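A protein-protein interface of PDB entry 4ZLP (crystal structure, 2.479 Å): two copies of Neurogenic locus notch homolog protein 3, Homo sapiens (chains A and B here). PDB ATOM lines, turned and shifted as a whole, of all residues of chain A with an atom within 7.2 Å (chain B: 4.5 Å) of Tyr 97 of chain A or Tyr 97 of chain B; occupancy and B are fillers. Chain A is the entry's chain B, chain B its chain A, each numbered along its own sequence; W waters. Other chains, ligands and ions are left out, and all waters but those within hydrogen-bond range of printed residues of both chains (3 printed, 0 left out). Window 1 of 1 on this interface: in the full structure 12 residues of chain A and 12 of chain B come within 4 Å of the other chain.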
ATOM      1  N   PRO A  92       8.600 -10.912 -13.094  1.00  0.00           N
ATOM      2  CA  PRO A  92       7.407 -11.772 -13.146  1.00  0.00           C
ATOM      3  C   PRO A  92       7.385 -12.789 -12.022  1.00  0.00           C
ATOM      4  O   PRO A  92       6.319 -13.176 -11.549  1.00  0.00           O
ATOM      5  CB  PRO A  92       7.527 -12.465 -14.506  1.00  0.00           C
ATOM      6  CG  PRO A  92       8.351 -11.538 -15.325  1.00  0.00           C
ATOM      7  CD  PRO A  92       9.322 -10.891 -14.378  1.00  0.00           C
ATOM      8  N   VAL A  93       8.564 -13.202 -11.587  1.00  0.00           N
ATOM      9  CA  VAL A  93       8.661 -14.161 -10.502  1.00  0.00           C
ATOM     10  C   VAL A  93       8.212 -13.548  -9.165  1.00  0.00           C
ATOM     11  O   VAL A  93       7.656 -14.249  -8.319  1.00  0.00           O
ATOM     12  CB  VAL A  93      10.102 -14.713 -10.397  1.00  0.00           C
ATOM     13  CG1 VAL A  93      10.188 -15.787  -9.338  1.00  0.00           C
ATOM     14  CG2 VAL A  93      10.546 -15.284 -11.748  1.00  0.00           C
ATOM     15  N   TYR A  94       8.410 -12.240  -8.991  1.00  0.00           N
ATOM     16  CA  TYR A  94       8.092 -11.577  -7.717  1.00  0.00           C
ATOM     17  C   TYR A  94       6.791 -10.784  -7.767  1.00  0.00           C
ATOM     18  O   TYR A  94       6.295 -10.309  -6.737  1.00  0.00           O
ATOM     19  CB  TYR A  94       9.232 -10.640  -7.297  1.00  0.00           C
ATOM     20  CG  TYR A  94      10.583 -11.312  -7.264  1.00  0.00           C
ATOM     21  CD1 TYR A  94      10.703 -12.665  -6.959  1.00  0.00           C
ATOM     22  CD2 TYR A  94      11.736 -10.606  -7.586  1.00  0.00           C
ATOM     23  CE1 TYR A  94      11.938 -13.286  -6.948  1.00  0.00           C
ATOM     24  CE2 TYR A  94      12.975 -11.218  -7.572  1.00  0.00           C
ATOM     25  CZ  TYR A  94      13.071 -12.557  -7.253  1.00  0.00           C
ATOM     26  OH  TYR A  94      14.302 -13.172  -7.252  1.00  0.00           O
ATOM     27  N   GLU A  95       6.243 -10.652  -8.969  1.00  0.00           N
ATOM     28  CA  GLU A  95       5.105  -9.774  -9.210  1.00  0.00           C
ATOM     29  C   GLU A  95       3.909 -10.066  -8.307  1.00  0.00           C
ATOM     30  O   GLU A  95       3.299  -9.151  -7.774  1.00  0.00           O
ATOM     31  CB  GLU A  95       4.677  -9.862 -10.677  1.00  0.00           C
ATOM     32  CG  GLU A  95       3.280  -9.325 -10.935  1.00  0.00           C
ATOM     33  CD  GLU A  95       3.102  -7.887 -10.483  1.00  0.00           C
ATOM     34  OE1 GLU A  95       4.077  -7.108 -10.520  1.00  0.00           O
ATOM     35  OE2 GLU A  95       1.980  -7.539 -10.062  1.00  0.00           O
ATOM     36  N   LYS A  96       3.556 -11.333  -8.156  1.00  0.00           N
ATOM     37  CA  LYS A  96       2.401 -11.689  -7.345  1.00  0.00           C
ATOM     38  C   LYS A  96       2.605 -11.326  -5.873  1.00  0.00           C
ATOM     39  O   LYS A  96       1.682 -10.850  -5.208  1.00  0.00           O
ATOM     40  CB  LYS A  96       2.086 -13.172  -7.499  1.00  0.00           C
ATOM     41  CG  LYS A  96       0.911 -13.624  -6.671  1.00  0.00           C
ATOM     42  CD  LYS A  96      -0.403 -12.940  -7.005  1.00  0.00           C
ATOM     43  CE  LYS A  96      -1.539 -13.604  -6.231  1.00  0.00           C
ATOM     44  NZ  LYS A  96      -2.832 -12.879  -6.369  1.00  0.00           N
ATOM     45  N   TYR A  97       3.813 -11.541  -5.365  1.00  0.00           N
ATOM     46  CA  TYR A  97       4.136 -11.118  -4.008  1.00  0.00           C
ATOM     47  C   TYR A  97       4.002  -9.593  -3.842  1.00  0.00           C
ATOM     48  O   TYR A  97       3.398  -9.117  -2.872  1.00  0.00           O
ATOM     49  CB  TYR A  97       5.542 -11.563  -3.637  1.00  0.00           C
ATOM     50  CG  TYR A  97       6.018 -11.085  -2.275  1.00  0.00           C
ATOM     51  CD1 TYR A  97       6.508  -9.783  -2.098  1.00  0.00           C
ATOM     52  CD2 TYR A  97       6.003 -11.936  -1.173  1.00  0.00           C
ATOM     53  CE1 TYR A  97       6.951  -9.338  -0.867  1.00  0.00           C
ATOM     54  CE2 TYR A  97       6.457 -11.500   0.067  1.00  0.00           C
ATOM     55  CZ  TYR A  97       6.928 -10.200   0.210  1.00  0.00           C
ATOM     56  OH  TYR A  97       7.381  -9.762   1.425  1.00  0.00           O
ATOM     57  N   CYS A  98       4.590  -8.833  -4.768  1.00  0.00           N
ATOM     58  CA  CYS A  98       4.572  -7.379  -4.661  1.00  0.00           C
ATOM     59  C   CYS A  98       3.153  -6.845  -4.681  1.00  0.00           C
ATOM     60  O   CYS A  98       2.808  -5.949  -3.919  1.00  0.00           O
ATOM     61  CB  CYS A  98       5.387  -6.743  -5.784  1.00  0.00           C
ATOM     62  SG  CYS A  98       7.161  -7.086  -5.641  1.00  0.00           S
ATOM     63  N   ALA A  99       2.324  -7.432  -5.533  1.00  0.00           N
ATOM     64  CA  ALA A  99       0.931  -7.031  -5.654  1.00  0.00           C
ATOM     65  C   ALA A  99       0.174  -7.237  -4.354  1.00  0.00           C
ATOM     66  O   ALA A  99      -0.561  -6.361  -3.907  1.00  0.00           O
ATOM     67  CB  ALA A  99       0.256  -7.816  -6.776  1.00  0.00           C
ATOM     68  N   ASP A 100       0.383  -8.391  -3.732  1.00  0.00           N
ATOM     69  CA  ASP A 100      -0.339  -8.725  -2.522  1.00  0.00           C
ATOM     70  C   ASP A 100       0.141  -7.875  -1.354  1.00  0.00           C
ATOM     71  O   ASP A 100      -0.643  -7.583  -0.453  1.00  0.00           O
ATOM     72  CB  ASP A 100      -0.173 -10.211  -2.178  1.00  0.00           C
ATOM     73  CG  ASP A 100      -1.073 -11.124  -3.000  1.00  0.00           C
ATOM     74  OD1 ASP A 100      -1.701 -10.675  -3.979  1.00  0.00           O
ATOM     75  OD2 ASP A 100      -1.153 -12.320  -2.656  1.00  0.00           O
ATOM     76  N   HIS A 101       1.401  -7.438  -1.379  1.00  0.00           N
ATOM     77  CA  HIS A 101       1.954  -6.706  -0.232  1.00  0.00           C
ATOM     78  C   HIS A 101       2.066  -5.187  -0.459  1.00  0.00           C
ATOM     79  O   HIS A 101       2.597  -4.457   0.382  1.00  0.00           O
ATOM     80  CB  HIS A 101       3.328  -7.276   0.156  1.00  0.00           C
ATOM     81  CG  HIS A 101       3.278  -8.678   0.681  1.00  0.00           C
ATOM     82  ND1 HIS A 101       3.305  -9.784  -0.140  1.00  0.00           N
ATOM     83  CD2 HIS A 101       3.199  -9.153   1.948  1.00  0.00           C
ATOM     84  CE1 HIS A 101       3.246 -10.880   0.597  1.00  0.00           C
ATOM     85  NE2 HIS A 101       3.177 -10.526   1.867  1.00  0.00           N
ATOM     86  N   PHE A 102       1.525  -4.725  -1.580  1.00  0.00           N
ATOM     87  CA  PHE A 102       1.457  -3.305  -1.940  1.00  0.00           C
ATOM     88  C   PHE A 102       0.566  -2.521  -0.974  1.00  0.00           C
ATOM     89  O   PHE A 102      -0.591  -2.879  -0.758  1.00  0.00           O
ATOM     90  CB  PHE A 102       0.944  -3.189  -3.382  1.00  0.00           C
ATOM     91  CG  PHE A 102       0.745  -1.781  -3.882  1.00  0.00           C
ATOM     92  CD1 PHE A 102      -0.462  -1.115  -3.687  1.00  0.00           C
ATOM     93  CD2 PHE A 102       1.742  -1.142  -4.605  1.00  0.00           C
ATOM     94  CE1 PHE A 102      -0.660   0.169  -4.184  1.00  0.00           C
ATOM     95  CE2 PHE A 102       1.547   0.140  -5.111  1.00  0.00           C
ATOM     96  CZ  PHE A 102       0.347   0.796  -4.892  1.00  0.00           C
ATOM     97  N   ASP A 104       0.453  -2.254   2.304  1.00  0.00           N
ATOM     98  CA  ASP A 104      -0.093  -3.000   3.429  1.00  0.00           C
ATOM     99  C   ASP A 104       0.451  -2.420   4.723  1.00  0.00           C
ATOM    100  O   ASP A 104       0.211  -2.957   5.800  1.00  0.00           O
ATOM    101  CB  ASP A 104       0.243  -4.486   3.320  1.00  0.00           C
ATOM    102  CG  ASP A 104       1.747  -4.758   3.286  1.00  0.00           C
ATOM    103  OD1 ASP A 104       2.561  -3.806   3.172  1.00  0.00           O
ATOM    104  OD2 ASP A 104       2.112  -5.948   3.375  1.00  0.00           O
ATOM    105  N   CYS A 107       7.041  -2.350   5.162  1.00  0.00           N
ATOM    106  CA  CYS A 107       8.005  -2.174   4.089  1.00  0.00           C
ATOM    107  C   CYS A 107       8.517  -3.495   3.512  1.00  0.00           C
ATOM    108  O   CYS A 107       9.036  -4.348   4.234  1.00  0.00           O
ATOM    109  CB  CYS A 107       9.182  -1.336   4.575  1.00  0.00           C
ATOM    110  SG  CYS A 107      10.416  -1.025   3.293  1.00  0.00           S
ATOM    111  N   ASP A 108       8.359  -3.655   2.200  1.00  0.00           N
ATOM    112  CA  ASP A 108       8.938  -4.786   1.496  1.00  0.00           C
ATOM    113  C   ASP A 108       9.995  -4.296   0.517  1.00  0.00           C
ATOM    114  O   ASP A 108       9.696  -4.008  -0.640  1.00  0.00           O
ATOM    115  CB  ASP A 108       7.867  -5.571   0.753  1.00  0.00           C
ATOM    116  CG  ASP A 108       6.820  -6.146   1.673  1.00  0.00           C
ATOM    117  OD1 ASP A 108       7.051  -7.263   2.187  1.00  0.00           O
ATOM    118  OD2 ASP A 108       5.757  -5.504   1.855  1.00  0.00           O
ATOM    119  N   GLN A 109      11.242  -4.255   0.962  1.00  0.00           N
ATOM    120  CA  GLN A 109      12.294  -3.633   0.166  1.00  0.00           C
ATOM    121  C   GLN A 109      12.461  -4.242  -1.226  1.00  0.00           C
ATOM    122  O   GLN A 109      12.835  -3.543  -2.150  1.00  0.00           O
ATOM    123  CB  GLN A 109      13.626  -3.722   0.905  1.00  0.00           C
ATOM    124  CG  GLN A 109      13.755  -2.779   2.072  1.00  0.00           C
ATOM    125  CD  GLN A 109      13.792  -1.304   1.659  1.00  0.00           C
ATOM    126  OE1 GLN A 109      13.970  -0.961   0.480  1.00  0.00           O
ATOM    127  NE2 GLN A 109      13.657  -0.428   2.644  1.00  0.00           N
ATOM    128  N   GLY A 110      12.164  -5.532  -1.383  1.00  0.00           N
ATOM    129  CA  GLY A 110      12.329  -6.199  -2.669  1.00  0.00           C
ATOM    130  C   GLY A 110      11.338  -5.713  -3.713  1.00  0.00           C
ATOM    131  O   GLY A 110      11.547  -5.876  -4.910  1.00  0.00           O
ATOM    132  N   CYS A 111      10.261  -5.095  -3.244  1.00  0.00           N
ATOM    133  CA  CYS A 111       9.239  -4.506  -4.103  1.00  0.00           C
ATOM    134  C   CYS A 111       9.395  -2.980  -4.152  1.00  0.00           C
ATOM    135  O   CYS A 111       8.649  -2.285  -4.834  1.00  0.00           O
ATOM    136  CB  CYS A 111       7.838  -4.882  -3.602  1.00  0.00           C
ATOM    137  SG  CYS A 111       7.457  -6.650  -3.661  1.00  0.00           S
ATOM    138  N   ASN A 112      10.383  -2.466  -3.430  1.00  0.00           N
ATOM    139  CA  ASN A 112      10.589  -1.029  -3.329  1.00  0.00           C
ATOM    140  C   ASN A 112      11.326  -0.419  -4.535  1.00  0.00           C
ATOM    141  O   ASN A 112      12.425   0.120  -4.388  1.00  0.00           O
ATOM    142  CB  ASN A 112      11.342  -0.723  -2.036  1.00  0.00           C
ATOM    143  CG  ASN A 112      11.375   0.746  -1.706  1.00  0.00           C
ATOM    144  OD1 ASN A 112      10.530   1.525  -2.157  1.00  0.00           O
ATOM    145  ND2 ASN A 112      12.333   1.134  -0.878  1.00  0.00           N
ATOM    146  N   ASP A 119       6.193  -0.417  -3.515  1.00  0.00           N
ATOM    147  CA  ASP A 119       5.511  -1.071  -2.381  1.00  0.00           C
ATOM    148  C   ASP A 119       4.387  -0.205  -1.819  1.00  0.00           C
ATOM    149  O   ASP A 119       4.078  -0.254  -0.619  1.00  0.00           O
ATOM    150  CB  ASP A 119       6.501  -1.433  -1.252  1.00  0.00           C
ATOM    151  CG  ASP A 119       5.902  -2.408  -0.218  1.00  0.00           C
ATOM    152  OD1 ASP A 119       5.038  -3.235  -0.574  1.00  0.00           O
ATOM    153  OD2 ASP A 119       6.279  -2.354   0.968  1.00  0.00           O
ATOM    154  N   GLN A 156      -1.303  -1.754  -7.570  1.00  0.00           N
ATOM    155  CA  GLN A 156       0.104  -2.103  -7.749  1.00  0.00           C
ATOM    156  C   GLN A 156       0.458  -2.225  -9.220  1.00  0.00           C
ATOM    157  O   GLN A 156       1.488  -1.716  -9.670  1.00  0.00           O
ATOM    158  CB  GLN A 156       0.455  -3.409  -7.035  1.00  0.00           C
ATOM    159  CG  GLN A 156       1.955  -3.730  -7.029  1.00  0.00           C
ATOM    160  CD  GLN A 156       2.396  -4.600  -8.188  1.00  0.00           C
ATOM    161  OE1 GLN A 156       1.576  -5.242  -8.843  1.00  0.00           O
ATOM    162  NE2 GLN A 156       3.710  -4.656  -8.422  1.00  0.00           N
ATOM    163  N   TYR B  94       4.177 -17.032  -2.121  1.00  0.00           N
ATOM    164  CA  TYR B  94       5.209 -16.070  -1.742  1.00  0.00           C
ATOM    165  C   TYR B  94       6.568 -16.730  -1.545  1.00  0.00           C
ATOM    166  O   TYR B  94       7.573 -16.042  -1.385  1.00  0.00           O
ATOM    167  CB  TYR B  94       4.822 -15.324  -0.465  1.00  0.00           C
ATOM    168  CG  TYR B  94       3.442 -14.678  -0.488  1.00  0.00           C
ATOM    169  CD1 TYR B  94       2.864 -14.242  -1.679  1.00  0.00           C
ATOM    170  CD2 TYR B  94       2.726 -14.497   0.696  1.00  0.00           C
ATOM    171  CE1 TYR B  94       1.613 -13.652  -1.686  1.00  0.00           C
ATOM    172  CE2 TYR B  94       1.479 -13.910   0.701  1.00  0.00           C
ATOM    173  CZ  TYR B  94       0.925 -13.492  -0.484  1.00  0.00           C
ATOM    174  OH  TYR B  94      -0.317 -12.911  -0.464  1.00  0.00           O
ATOM    175  N   GLU B  95       6.587 -18.062  -1.562  1.00  0.00           N
ATOM    176  CA  GLU B  95       7.772 -18.844  -1.206  1.00  0.00           C
ATOM    177  C   GLU B  95       8.997 -18.507  -2.065  1.00  0.00           C
ATOM    178  O   GLU B  95      10.093 -18.285  -1.540  1.00  0.00           O
ATOM    179  CB  GLU B  95       7.457 -20.349  -1.301  1.00  0.00           C
ATOM    180  CG  GLU B  95       8.678 -21.269  -1.336  1.00  0.00           C
ATOM    181  CD  GLU B  95       9.609 -21.116  -0.123  1.00  0.00           C
ATOM    182  OE1 GLU B  95      10.824 -21.375  -0.281  1.00  0.00           O
ATOM    183  OE2 GLU B  95       9.141 -20.772   0.990  1.00  0.00           O
ATOM    184  N   LYS B  96       8.803 -18.435  -3.379  1.00  0.00           N
ATOM    185  CA  LYS B  96       9.921 -18.181  -4.270  1.00  0.00           C
ATOM    186  C   LYS B  96      10.513 -16.801  -3.982  1.00  0.00           C
ATOM    187  O   LYS B  96      11.734 -16.651  -3.907  1.00  0.00           O
ATOM    188  CB  LYS B  96       9.478 -18.277  -5.727  1.00  0.00           C
ATOM    189  CG  LYS B  96      10.591 -18.085  -6.739  1.00  0.00           C
ATOM    190  CD  LYS B  96      11.635 -19.176  -6.574  1.00  0.00           C
ATOM    191  CE  LYS B  96      12.657 -19.173  -7.701  1.00  0.00           C
ATOM    192  NZ  LYS B  96      13.555 -17.993  -7.642  1.00  0.00           N
ATOM    193  N   TYR B  97       9.647 -15.809  -3.767  1.00  0.00           N
ATOM    194  CA  TYR B  97      10.107 -14.473  -3.391  1.00  0.00           C
ATOM    195  C   TYR B  97      10.892 -14.515  -2.063  1.00  0.00           C
ATOM    196  O   TYR B  97      11.981 -13.942  -1.970  1.00  0.00           O
ATOM    197  CB  TYR B  97       8.934 -13.499  -3.282  1.00  0.00           C
ATOM    198  CG  TYR B  97       9.320 -12.095  -2.830  1.00  0.00           C
ATOM    199  CD1 TYR B  97       9.541 -11.808  -1.491  1.00  0.00           C
ATOM    200  CD2 TYR B  97       9.449 -11.048  -3.758  1.00  0.00           C
ATOM    201  CE1 TYR B  97       9.915 -10.533  -1.077  1.00  0.00           C
ATOM    202  CE2 TYR B  97       9.806  -9.751  -3.352  1.00  0.00           C
ATOM    203  CZ  TYR B  97      10.032  -9.507  -2.006  1.00  0.00           C
ATOM    204  OH  TYR B  97      10.380  -8.250  -1.577  1.00  0.00           O
ATOM    205  N   CYS B  98      10.338 -15.171  -1.042  1.00  0.00           N
ATOM    206  CA  CYS B  98      11.003 -15.236   0.260  1.00  0.00           C
ATOM    207  C   CYS B  98      12.369 -15.932   0.197  1.00  0.00           C
ATOM    208  O   CYS B  98      13.339 -15.474   0.802  1.00  0.00           O
ATOM    209  CB  CYS B  98      10.095 -15.930   1.285  1.00  0.00           C
ATOM    210  SG  CYS B  98       8.631 -14.909   1.719  1.00  0.00           S
ATOM    211  N   ALA B  99      12.447 -17.011  -0.572  1.00  0.00           N
ATOM    212  CA  ALA B  99      13.699 -17.741  -0.737  1.00  0.00           C
ATOM    213  C   ALA B  99      14.751 -16.839  -1.383  1.00  0.00           C
ATOM    214  O   ALA B  99      15.910 -16.844  -0.968  1.00  0.00           O
ATOM    215  CB  ALA B  99      13.483 -19.011  -1.562  1.00  0.00           C
ATOM    216  N   ASP B 100      14.346 -16.072  -2.393  1.00  0.00           N
ATOM    217  CA  ASP B 100      15.269 -15.184  -3.099  1.00  0.00           C
ATOM    218  C   ASP B 100      15.690 -13.948  -2.303  1.00  0.00           C
ATOM    219  O   ASP B 100      16.757 -13.396  -2.557  1.00  0.00           O
ATOM    220  CB  ASP B 100      14.664 -14.733  -4.422  1.00  0.00           C
ATOM    221  CG  ASP B 100      14.790 -15.785  -5.500  1.00  0.00           C
ATOM    222  OD1 ASP B 100      15.189 -16.916  -5.156  1.00  0.00           O
ATOM    223  OD2 ASP B 100      14.471 -15.487  -6.676  1.00  0.00           O
ATOM    224  N   HIS B 101      14.863 -13.497  -1.361  1.00  0.00           N
ATOM    225  CA  HIS B 101      15.180 -12.269  -0.629  1.00  0.00           C
ATOM    226  C   HIS B 101      15.655 -12.536   0.802  1.00  0.00           C
ATOM    227  O   HIS B 101      15.841 -11.607   1.598  1.00  0.00           O
ATOM    228  CB  HIS B 101      13.967 -11.334  -0.646  1.00  0.00           C
ATOM    229  CG  HIS B 101      13.639 -10.840  -2.017  1.00  0.00           C
ATOM    230  ND1 HIS B 101      12.849 -11.551  -2.890  1.00  0.00           N
ATOM    231  CD2 HIS B 101      14.060  -9.747  -2.697  1.00  0.00           C
ATOM    232  CE1 HIS B 101      12.768 -10.901  -4.039  1.00  0.00           C
ATOM    233  NE2 HIS B 101      13.490  -9.801  -3.947  1.00  0.00           N
ATOM    234  N   ASP B 108      12.324  -7.422   4.327  1.00  0.00           N
ATOM    235  CA  ASP B 108      11.077  -7.739   3.650  1.00  0.00           C
ATOM    236  C   ASP B 108      10.047  -8.232   4.655  1.00  0.00           C
ATOM    237  O   ASP B 108      10.041  -9.412   5.015  1.00  0.00           O
ATOM    238  CB  ASP B 108      11.290  -8.798   2.569  1.00  0.00           C
ATOM    239  CG  ASP B 108      12.286  -8.365   1.517  1.00  0.00           C
ATOM    240  OD1 ASP B 108      11.884  -7.697   0.540  1.00  0.00           O
ATOM    241  OD2 ASP B 108      13.477  -8.714   1.661  1.00  0.00           O
ATOM    242  N   GLY B 110       6.990  -8.951   4.557  1.00  0.00           N
ATOM    243  CA  GLY B 110       6.066  -9.983   4.117  1.00  0.00           C
ATOM    244  C   GLY B 110       6.630 -11.383   4.298  1.00  0.00           C
ATOM    245  O   GLY B 110       5.903 -12.371   4.290  1.00  0.00           O
ATOM    246  N   CYS B 111       7.947 -11.467   4.447  1.00  0.00           N
ATOM    247  CA  CYS B 111       8.618 -12.731   4.714  1.00  0.00           C
ATOM    248  C   CYS B 111       9.073 -12.786   6.173  1.00  0.00           C
ATOM    249  O   CYS B 111       9.674 -13.758   6.613  1.00  0.00           O
ATOM    250  CB  CYS B 111       9.815 -12.910   3.764  1.00  0.00           C
ATOM    251  SG  CYS B 111       9.365 -13.010   2.005  1.00  0.00           S
HETATM  252  O   HOH W   1       4.178  -6.932   4.418  1.00  0.00           O
HETATM  253  O   HOH W   2      13.637  -7.524  -6.084  1.00  0.00           O
HETATM  254  O   HOH W   3       2.845 -12.345   4.347  1.00  0.00           O
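Water W1 lies within hydrogen-bond range of the side-chain carboxylate (OD2) of Asp 104 of chain A (2.5 Å) and the backbone NH (N) of Gly 110 of chain B (3.5 Å).
Water W2 bridges O of Gly 110 of chain A (2.9 Å) and NE2 of His 101 of chain B (3.1 Å).
Water W3 bridges O of Gly 110 of chain B (3.1 Å) and NE2 of His 101 of chain A (3.1 Å).
A ring nitrogen (ND1) of His 101 of chain A sits at hydrogen-bond distance from the backbone carbonyl oxygen (O) of Tyr 97 of chain A (2.8 Å).
NZ of Lys 96 of chain B lies within salt-bridge range of OD2 of Asp 100 of chain B (2.8 Å).
SG of Cys 111 of chain A forms a disulfide with SG of Cys 98 of chain A (2.0 Å).
SG of Cys 107 of chain A is in hydrogen-bond range of NE2 of Gln 109 of chain A (3.4 Å).
The side-chain hydroxyl (OH) of Tyr 97 of chain B is in hydrogen-bond range of the side-chain carboxylate (OD1) of Asp 108 of chain B, 2.7 Å away.
A ring nitrogen (ND1) of His 101 of chain B lies within hydrogen-bond range of the backbone carbonyl oxygen of Tyr 97 of chain B, 2.7 Å away.
CD2 of Tyr 97 of chain B touches CB of Tyr 94 of chain A, at 3.6 Å.
Tyr 94 of chain A touches His 101 of chain B.
Tyr 97 of chain A touches Tyr 94 of chain B (CD2 to CB, 3.7 Å).
CE1 of Tyr 97 of chain A touches CE1 of Tyr 97 of chain B, at 3.2 Å.
His 101 of chain A touches Tyr 94 of chain B (CE1 to CE2, 3.5 Å).
His 101 of chain A touches Gly 110 of chain B (CD2 to CA, 3.7 Å).
Asp 108 of chain A touches Asp 108 of chain B (C to OD1, 3.9 Å).
N of Gln 109 of chain A touches OD1 of Asp 108 of chain B (3.5 Å).
Gly 110 of chain A touches His 101 of chain B.
N of Cys 111 of chain A touches OH of Tyr 97 of chain B, 3.6 Å away.
Tyr 94 of chain A touches Tyr 97 of chain B, and with the chains exchanged Tyr 97 of chain A touches Tyr 94 of chain B.
Tyr 94 of chain A touches His 101 of chain B, and with the chains exchanged His 101 of chain A touches Tyr 94 of chain B.
His 101 of chain A touches Gly 110 of chain B, and with the chains exchanged Gly 110 of chain A touches His 101 of chain B.
Asp 108 of chain A touches Gly 110 of chain B, and with the chains exchanged Gly 110 of chain A touches Asp 108 of chain B.
Of the 18 pairs that touch across the chains among the printed residues, 16 have their exchanged pair printed and touching as well.
The side-chain hydroxyl (OH) of Tyr 97 of chain A sits close to the backbone NH (N) of Gly 110 of chain B, 3.3 Å away.
The side-chain hydroxyl of Tyr 94 of chain A lies close to the side-chain carboxylate of Asp 100 of chain B (2.4 Å).
The backbone NH (N) of Gly 110 of chain B sits at hydrogen-bond distance from the side-chain carboxylate (OD1) of Asp 108 of chain A, 2.9 Å away.
OH of Tyr 97 of chain B lies close to N of Gly 110 of chain A (3.3 Å).
OH of Tyr 94 of chain B is in hydrogen-bond range of OD2 of Asp 100 of chain A.
The side-chain carboxylate (OD1) of Asp 108 of chain B is in hydrogen-bond range of the backbone NH (N) of Gly 110 of chain A, 2.9 Å away.
Hydrophobic or aromatic side chains of chain A that line the printed part of chain B: Val 93, Tyr 94, Tyr 97 and His 101.
Of the 11 printed residues of chain B, 8 touch a printed residue of chain A.
Hydrophobic or aromatic side chains of chain B within 4 Å of the printed part of chain A: Tyr 94, Tyr 97 and His 101.
Among the printed residues, no Asp or Glu carboxylate lies within 4 Å of a Lys or Arg side-chain nitrogen of the other chain.
Of chain B, only Tyr 94, Tyr 97, Gly 110 and Cys 111 come within 4 Å of Tyr 97 of chain A.
Tyr 97 of chain B touches just these residues of chain A: Tyr 94 (3.6 Å), Tyr 97 (3.2 Å), Gly 110 (3.0 Å) and Cys 111 (3.6 Å).
Of the printed residues of chain A, Tyr 94 of chain B touches Tyr 97, Asp 100 and His 101.
Of the printed residues of chain A, Gly 110 of chain B touches Tyr 97 (3.0 Å), His 101 (3.7 Å) and Asp 108 (2.9 Å).
Of the printed residues of chain B, Gln 109 of chain A touches Asp 108 (3.5 Å).
Glu 95 of chain A touches none of the printed residues of chain B.
The nearest residue of chain B that does not touch Tyr 97 of chain A is Asp 108 of chain B (4.2 Å).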
